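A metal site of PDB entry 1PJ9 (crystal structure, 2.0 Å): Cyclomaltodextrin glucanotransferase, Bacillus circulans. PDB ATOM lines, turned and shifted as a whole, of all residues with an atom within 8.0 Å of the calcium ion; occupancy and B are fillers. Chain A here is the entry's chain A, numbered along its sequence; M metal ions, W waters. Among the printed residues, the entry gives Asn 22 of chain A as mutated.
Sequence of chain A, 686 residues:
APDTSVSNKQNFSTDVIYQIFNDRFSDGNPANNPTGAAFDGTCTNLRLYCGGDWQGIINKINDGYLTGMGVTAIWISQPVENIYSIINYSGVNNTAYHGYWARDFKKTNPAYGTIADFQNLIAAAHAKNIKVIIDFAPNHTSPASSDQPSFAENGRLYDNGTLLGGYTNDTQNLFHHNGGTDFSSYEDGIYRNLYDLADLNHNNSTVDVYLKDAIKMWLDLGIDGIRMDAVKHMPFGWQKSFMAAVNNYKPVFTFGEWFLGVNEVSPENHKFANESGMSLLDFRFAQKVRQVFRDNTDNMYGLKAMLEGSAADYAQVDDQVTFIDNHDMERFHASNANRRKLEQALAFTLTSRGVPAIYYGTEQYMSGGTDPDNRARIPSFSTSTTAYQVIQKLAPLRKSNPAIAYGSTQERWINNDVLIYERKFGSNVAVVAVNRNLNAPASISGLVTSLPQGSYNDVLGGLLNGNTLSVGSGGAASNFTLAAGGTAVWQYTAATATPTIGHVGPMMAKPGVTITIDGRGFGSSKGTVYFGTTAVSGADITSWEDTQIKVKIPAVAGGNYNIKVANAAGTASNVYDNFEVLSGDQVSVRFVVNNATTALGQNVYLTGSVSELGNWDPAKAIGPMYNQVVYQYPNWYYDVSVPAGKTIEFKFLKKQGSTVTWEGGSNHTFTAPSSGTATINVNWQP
The backbone NH of Gly 56 lies within hydrogen-bond range of the side-chain carboxylate of Asp 53 (2.8 Å).
The backbone NH (N) of Asp 53 lies within hydrogen-bond range of the backbone carbonyl oxygen (O) of Ser 26 (3.0 Å).
The backbone NH of Gln 55 is in hydrogen-bond range of the side-chain carboxylate of Asp 53, 3.2 Å away.
The side-chain amide oxygen (OD1) of Asn 29 sits at hydrogen-bond distance from the backbone NH (N) of Ala 31, at 3.0 Å.
O of Ala 111 lies close to OD1 of Asn 32 (3.2 Å).
The side-chain amide nitrogen of Asn 33 lies close to the backbone carbonyl oxygen of Pro 30 (3.3 Å).
OD1 of Asp 53 lies within hydrogen-bond range of N of Gly 28 (2.9 Å).
OD1 of Asp 23 lies within hydrogen-bond range of N of Gly 51.
Of the 24 residues printed, 6 come within 4 Å of the calcium ion.
The nearest printed residue that does not touch the calcium ion is Ala 111 (4.2 Å).
The calcium ion is bound by the side-chain amide oxygen (OD1) of Asn 33, the side-chain amide oxygen (OD1) of Asn 32, the side-chain carboxylate (OD2) of Asp 53, water W1, the side-chain carboxylate (OD1) of Asp 27, the backbone carbonyl oxygen (O) of Gly 51 and the backbone carbonyl oxygen (O) of Asn 29.
The calcium ion has seven donor atoms within binding distance.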
ATOM      1  N   ASN A  22      15.942  10.122 -22.176  1.00  0.00           N
ATOM      2  CA  ASN A  22      14.958  10.858 -22.973  1.00  0.00           C
ATOM      3  C   ASN A  22      15.048  12.372 -22.952  1.00  0.00           C
ATOM      4  O   ASN A  22      15.187  13.022 -23.986  1.00  0.00           O
ATOM      5  CB  ASN A  22      13.544  10.436 -22.563  1.00  0.00           C
ATOM      6  CG  ASN A  22      13.252   8.988 -22.878  1.00  0.00           C
ATOM      7  OD1 ASN A  22      14.145   8.232 -23.246  1.00  0.00           O
ATOM      8  ND2 ASN A  22      11.981   8.594 -22.742  1.00  0.00           N
ATOM      9  N   ASP A  23      14.948  12.945 -21.752  1.00  0.00           N
ATOM     10  CA  ASP A  23      14.951  14.390 -21.592  1.00  0.00           C
ATOM     11  C   ASP A  23      16.190  15.114 -22.108  1.00  0.00           C
ATOM     12  O   ASP A  23      16.114  16.290 -22.481  1.00  0.00           O
ATOM     13  CB  ASP A  23      14.750  14.743 -20.109  1.00  0.00           C
ATOM     14  CG  ASP A  23      14.506  16.220 -19.884  1.00  0.00           C
ATOM     15  OD1 ASP A  23      13.492  16.727 -20.415  1.00  0.00           O
ATOM     16  OD2 ASP A  23      15.322  16.872 -19.198  1.00  0.00           O
ATOM     17  N   SER A  26      16.838  14.508 -27.373  1.00  0.00           N
ATOM     18  CA  SER A  26      16.313  15.394 -28.412  1.00  0.00           C
ATOM     19  C   SER A  26      14.850  15.798 -28.212  1.00  0.00           C
ATOM     20  O   SER A  26      13.972  14.940 -28.119  1.00  0.00           O
ATOM     21  CB  SER A  26      16.466  14.742 -29.782  1.00  0.00           C
ATOM     22  OG  SER A  26      16.030  15.618 -30.814  1.00  0.00           O
ATOM     23  N   ASP A  27      14.609  17.102 -28.156  1.00  0.00           N
ATOM     24  CA  ASP A  27      13.261  17.644 -28.009  1.00  0.00           C
ATOM     25  C   ASP A  27      12.635  17.742 -29.398  1.00  0.00           C
ATOM     26  O   ASP A  27      12.840  18.715 -30.114  1.00  0.00           O
ATOM     27  CB  ASP A  27      13.326  19.019 -27.340  1.00  0.00           C
ATOM     28  CG  ASP A  27      11.963  19.662 -27.146  1.00  0.00           C
ATOM     29  OD1 ASP A  27      10.924  18.973 -27.292  1.00  0.00           O
ATOM     30  OD2 ASP A  27      11.924  20.870 -26.822  1.00  0.00           O
ATOM     31  N   GLY A  28      11.879  16.710 -29.776  1.00  0.00           N
ATOM     32  CA  GLY A  28      11.248  16.695 -31.083  1.00  0.00           C
ATOM     33  C   GLY A  28       9.882  17.357 -31.108  1.00  0.00           C
ATOM     34  O   GLY A  28       9.352  17.651 -32.181  1.00  0.00           O
ATOM     35  N   ASN A  29       9.305  17.571 -29.933  1.00  0.00           N
ATOM     36  CA  ASN A  29       7.996  18.213 -29.831  1.00  0.00           C
ATOM     37  C   ASN A  29       7.987  19.192 -28.665  1.00  0.00           C
ATOM     38  O   ASN A  29       7.738  18.807 -27.525  1.00  0.00           O
ATOM     39  CB  ASN A  29       6.900  17.160 -29.633  1.00  0.00           C
ATOM     40  CG  ASN A  29       5.514  17.780 -29.517  1.00  0.00           C
ATOM     41  OD1 ASN A  29       5.343  18.987 -29.688  1.00  0.00           O
ATOM     42  ND2 ASN A  29       4.519  16.959 -29.200  1.00  0.00           N
ATOM     43  N   PRO A  30       8.257  20.484 -28.937  1.00  0.00           N
ATOM     44  CA  PRO A  30       8.277  21.525 -27.905  1.00  0.00           C
ATOM     45  C   PRO A  30       6.930  21.698 -27.206  1.00  0.00           C
ATOM     46  O   PRO A  30       6.864  22.219 -26.088  1.00  0.00           O
ATOM     47  CB  PRO A  30       8.680  22.781 -28.677  1.00  0.00           C
ATOM     48  CG  PRO A  30       9.470  22.225 -29.830  1.00  0.00           C
ATOM     49  CD  PRO A  30       8.648  21.042 -30.244  1.00  0.00           C
ATOM     50  N   ALA A  31       5.868  21.256 -27.865  1.00  0.00           N
ATOM     51  CA  ALA A  31       4.510  21.393 -27.330  1.00  0.00           C
ATOM     52  C   ALA A  31       4.249  20.611 -26.039  1.00  0.00           C
ATOM     53  O   ALA A  31       3.385  20.999 -25.250  1.00  0.00           O
ATOM     54  CB  ALA A  31       3.486  21.002 -28.395  1.00  0.00           C
ATOM     55  N   ASN A  32       4.968  19.516 -25.820  1.00  0.00           N
ATOM     56  CA  ASN A  32       4.764  18.725 -24.615  1.00  0.00           C
ATOM     57  C   ASN A  32       5.746  19.053 -23.486  1.00  0.00           C
ATOM     58  O   ASN A  32       5.762  18.372 -22.459  1.00  0.00           O
ATOM     59  CB  ASN A  32       4.816  17.222 -24.916  1.00  0.00           C
ATOM     60  CG  ASN A  32       6.131  16.790 -25.548  1.00  0.00           C
ATOM     61  OD1 ASN A  32       7.191  17.339 -25.243  1.00  0.00           O
ATOM     62  ND2 ASN A  32       6.073  15.787 -26.422  1.00  0.00           N
ATOM     63  N   ASN A  33       6.557  20.094 -23.683  1.00  0.00           N
ATOM     64  CA  ASN A  33       7.529  20.481 -22.670  1.00  0.00           C
ATOM     65  C   ASN A  33       6.872  20.993 -21.397  1.00  0.00           C
ATOM     66  O   ASN A  33       5.904  21.750 -21.442  1.00  0.00           O
ATOM     67  CB  ASN A  33       8.464  21.581 -23.178  1.00  0.00           C
ATOM     68  CG  ASN A  33       9.316  21.151 -24.349  1.00  0.00           C
ATOM     69  OD1 ASN A  33       9.424  19.959 -24.653  1.00  0.00           O
ATOM     70  ND2 ASN A  33       9.947  22.115 -25.012  1.00  0.00           N
ATOM     71  N   PRO A  34       7.382  20.564 -20.230  1.00  0.00           N
ATOM     72  CA  PRO A  34       6.801  21.065 -18.981  1.00  0.00           C
ATOM     73  C   PRO A  34       7.030  22.571 -19.000  1.00  0.00           C
ATOM     74  O   PRO A  34       7.831  23.064 -19.793  1.00  0.00           O
ATOM     75  CB  PRO A  34       7.617  20.348 -17.920  1.00  0.00           C
ATOM     76  CG  PRO A  34       7.893  19.020 -18.572  1.00  0.00           C
ATOM     77  CD  PRO A  34       8.293  19.433 -19.971  1.00  0.00           C
ATOM     78  N   PHE A  39      10.986  23.693 -15.923  1.00  0.00           N
ATOM     79  CA  PHE A  39      11.602  23.645 -17.233  1.00  0.00           C
ATOM     80  C   PHE A  39      12.736  24.641 -17.483  1.00  0.00           C
ATOM     81  O   PHE A  39      12.720  25.772 -17.003  1.00  0.00           O
ATOM     82  CB  PHE A  39      10.508  23.861 -18.291  1.00  0.00           C
ATOM     83  CG  PHE A  39      10.999  23.817 -19.712  1.00  0.00           C
ATOM     84  CD1 PHE A  39      11.325  22.596 -20.307  1.00  0.00           C
ATOM     85  CD2 PHE A  39      11.122  24.979 -20.457  1.00  0.00           C
ATOM     86  CE1 PHE A  39      11.769  22.536 -21.626  1.00  0.00           C
ATOM     87  CE2 PHE A  39      11.559  24.935 -21.787  1.00  0.00           C
ATOM     88  CZ  PHE A  39      11.884  23.710 -22.369  1.00  0.00           C
ATOM     89  N   TYR A  49      13.406  19.780 -16.338  1.00  0.00           N
ATOM     90  CA  TYR A  49      13.144  19.208 -17.662  1.00  0.00           C
ATOM     91  C   TYR A  49      13.810  20.063 -18.725  1.00  0.00           C
ATOM     92  O   TYR A  49      13.735  21.298 -18.681  1.00  0.00           O
ATOM     93  CB  TYR A  49      11.644  19.134 -17.955  1.00  0.00           C
ATOM     94  CG  TYR A  49      10.936  17.916 -17.401  1.00  0.00           C
ATOM     95  CD1 TYR A  49      10.382  17.918 -16.121  1.00  0.00           C
ATOM     96  CD2 TYR A  49      10.775  16.773 -18.176  1.00  0.00           C
ATOM     97  CE1 TYR A  49       9.690  16.805 -15.627  1.00  0.00           C
ATOM     98  CE2 TYR A  49      10.084  15.664 -17.696  1.00  0.00           C
ATOM     99  CZ  TYR A  49       9.545  15.689 -16.429  1.00  0.00           C
ATOM    100  OH  TYR A  49       8.845  14.588 -15.970  1.00  0.00           O
ATOM    101  N   CYS A  50      14.442  19.412 -19.695  1.00  0.00           N
ATOM    102  CA  CYS A  50      15.110  20.098 -20.784  1.00  0.00           C
ATOM    103  C   CYS A  50      14.288  20.008 -22.070  1.00  0.00           C
ATOM    104  O   CYS A  50      14.495  20.791 -23.000  1.00  0.00           O
ATOM    105  CB  CYS A  50      16.505  19.505 -20.980  1.00  0.00           C
ATOM    106  SG  CYS A  50      17.632  19.954 -19.622  1.00  0.00           S
ATOM    107  N   GLY A  51      13.374  19.049 -22.128  1.00  0.00           N
ATOM    108  CA  GLY A  51      12.506  18.931 -23.294  1.00  0.00           C
ATOM    109  C   GLY A  51      12.601  17.654 -24.122  1.00  0.00           C
ATOM    110  O   GLY A  51      11.707  17.393 -24.934  1.00  0.00           O
ATOM    111  N   GLY A  52      13.665  16.882 -23.928  1.00  0.00           N
ATOM    112  CA  GLY A  52      13.848  15.651 -24.701  1.00  0.00           C
ATOM    113  C   GLY A  52      12.656  14.720 -24.623  1.00  0.00           C
ATOM    114  O   GLY A  52      12.141  14.454 -23.526  1.00  0.00           O
ATOM    115  N   ASP A  53      12.226  14.188 -25.765  1.00  0.00           N
ATOM    116  CA  ASP A  53      11.040  13.341 -25.793  1.00  0.00           C
ATOM    117  C   ASP A  53      11.092  12.214 -26.809  1.00  0.00           C
ATOM    118  O   ASP A  53      12.104  11.993 -27.472  1.00  0.00           O
ATOM    119  CB  ASP A  53       9.816  14.215 -26.061  1.00  0.00           C
ATOM    120  CG  ASP A  53       9.986  15.076 -27.292  1.00  0.00           C
ATOM    121  OD1 ASP A  53      10.556  14.583 -28.291  1.00  0.00           O
ATOM    122  OD2 ASP A  53       9.552  16.255 -27.270  1.00  0.00           O
ATOM    123  N   TRP A  54       9.970  11.503 -26.957  1.00  0.00           N
ATOM    124  CA  TRP A  54       9.903  10.385 -27.886  1.00  0.00           C
ATOM    125  C   TRP A  54       9.959  10.797 -29.347  1.00  0.00           C
ATOM    126  O   TRP A  54      10.558  10.103 -30.170  1.00  0.00           O
ATOM    127  CB  TRP A  54       8.643   9.543 -27.614  1.00  0.00           C
ATOM    128  CG  TRP A  54       8.679   8.819 -26.299  1.00  0.00           C
ATOM    129  CD1 TRP A  54       9.803   8.413 -25.624  1.00  0.00           C
ATOM    130  CD2 TRP A  54       7.561   8.405 -25.500  1.00  0.00           C
ATOM    131  NE1 TRP A  54       9.442   7.778 -24.452  1.00  0.00           N
ATOM    132  CE2 TRP A  54       8.077   7.759 -24.360  1.00  0.00           C
ATOM    133  CE3 TRP A  54       6.169   8.535 -25.646  1.00  0.00           C
ATOM    134  CZ2 TRP A  54       7.245   7.228 -23.358  1.00  0.00           C
ATOM    135  CZ3 TRP A  54       5.350   8.005 -24.649  1.00  0.00           C
ATOM    136  CH2 TRP A  54       5.892   7.362 -23.520  1.00  0.00           C
ATOM    137  N   GLN A  55       9.360  11.936 -29.687  1.00  0.00           N
ATOM    138  CA  GLN A  55       9.412  12.395 -31.072  1.00  0.00           C
ATOM    139  C   GLN A  55      10.860  12.681 -31.441  1.00  0.00           C
ATOM    140  O   GLN A  55      11.290  12.470 -32.580  1.00  0.00           O
ATOM    141  CB  GLN A  55       8.563  13.665 -31.255  1.00  0.00           C
ATOM    142  CG  GLN A  55       8.549  14.195 -32.685  1.00  0.00           C
ATOM    143  CD  GLN A  55       8.002  13.187 -33.691  1.00  0.00           C
ATOM    144  OE1 GLN A  55       8.685  12.805 -34.648  1.00  0.00           O
ATOM    145  NE2 GLN A  55       6.767  12.755 -33.482  1.00  0.00           N
ATOM    146  N   GLY A  56      11.630  13.156 -30.460  1.00  0.00           N
ATOM    147  CA  GLY A  56      13.032  13.431 -30.702  1.00  0.00           C
ATOM    148  C   GLY A  56      13.784  12.145 -31.024  1.00  0.00           C
ATOM    149  O   GLY A  56      14.628  12.122 -31.917  1.00  0.00           O
ATOM    150  N   PRO A 110       3.517  12.424 -19.949  1.00  0.00           N
ATOM    151  CA  PRO A 110       3.191  13.390 -21.005  1.00  0.00           C
ATOM    152  C   PRO A 110       4.352  14.200 -21.554  1.00  0.00           C
ATOM    153  O   PRO A 110       4.303  14.678 -22.698  1.00  0.00           O
ATOM    154  CB  PRO A 110       2.104  14.256 -20.353  1.00  0.00           C
ATOM    155  CG  PRO A 110       2.435  14.164 -18.891  1.00  0.00           C
ATOM    156  CD  PRO A 110       2.758  12.711 -18.724  1.00  0.00           C
ATOM    157  N   ALA A 111       5.406  14.365 -20.757  1.00  0.00           N
ATOM    158  CA  ALA A 111       6.578  15.105 -21.208  1.00  0.00           C
ATOM    159  C   ALA A 111       7.276  14.328 -22.332  1.00  0.00           C
ATOM    160  O   ALA A 111       7.798  14.922 -23.281  1.00  0.00           O
ATOM    161  CB  ALA A 111       7.544  15.329 -20.055  1.00  0.00           C
ATOM    162  N   TYR A 112       7.267  12.998 -22.237  1.00  0.00           N
ATOM    163  CA  TYR A 112       7.884  12.170 -23.276  1.00  0.00           C
ATOM    164  C   TYR A 112       6.931  12.043 -24.462  1.00  0.00           C
ATOM    165  O   TYR A 112       7.361  12.021 -25.620  1.00  0.00           O
ATOM    166  CB  TYR A 112       8.224  10.776 -22.743  1.00  0.00           C
ATOM    167  CG  TYR A 112       9.186  10.753 -21.561  1.00  0.00           C
ATOM    168  CD1 TYR A 112      10.049  11.810 -21.304  1.00  0.00           C
ATOM    169  CD2 TYR A 112       9.232   9.637 -20.713  1.00  0.00           C
ATOM    170  CE1 TYR A 112      10.938  11.779 -20.223  1.00  0.00           C
ATOM    171  CE2 TYR A 112      10.117   9.598 -19.643  1.00  0.00           C
ATOM    172  CZ  TYR A 112      10.966  10.666 -19.399  1.00  0.00           C
ATOM    173  OH  TYR A 112      11.821  10.615 -18.328  1.00  0.00           O
ATOM    174  N   GLY A 113       5.637  11.944 -24.171  1.00  0.00           N
ATOM    175  CA  GLY A 113       4.660  11.829 -25.228  1.00  0.00           C
ATOM    176  C   GLY A 113       3.399  11.087 -24.803  1.00  0.00           C
ATOM    177  O   GLY A 113       3.239  10.709 -23.650  1.00  0.00           O
HETATM  178 CA    CA M   1       9.373  17.994 -25.690  1.00  0.00          CA
HETATM  179  O   HOH W   1       9.213  17.191 -23.457  1.00  0.00           O
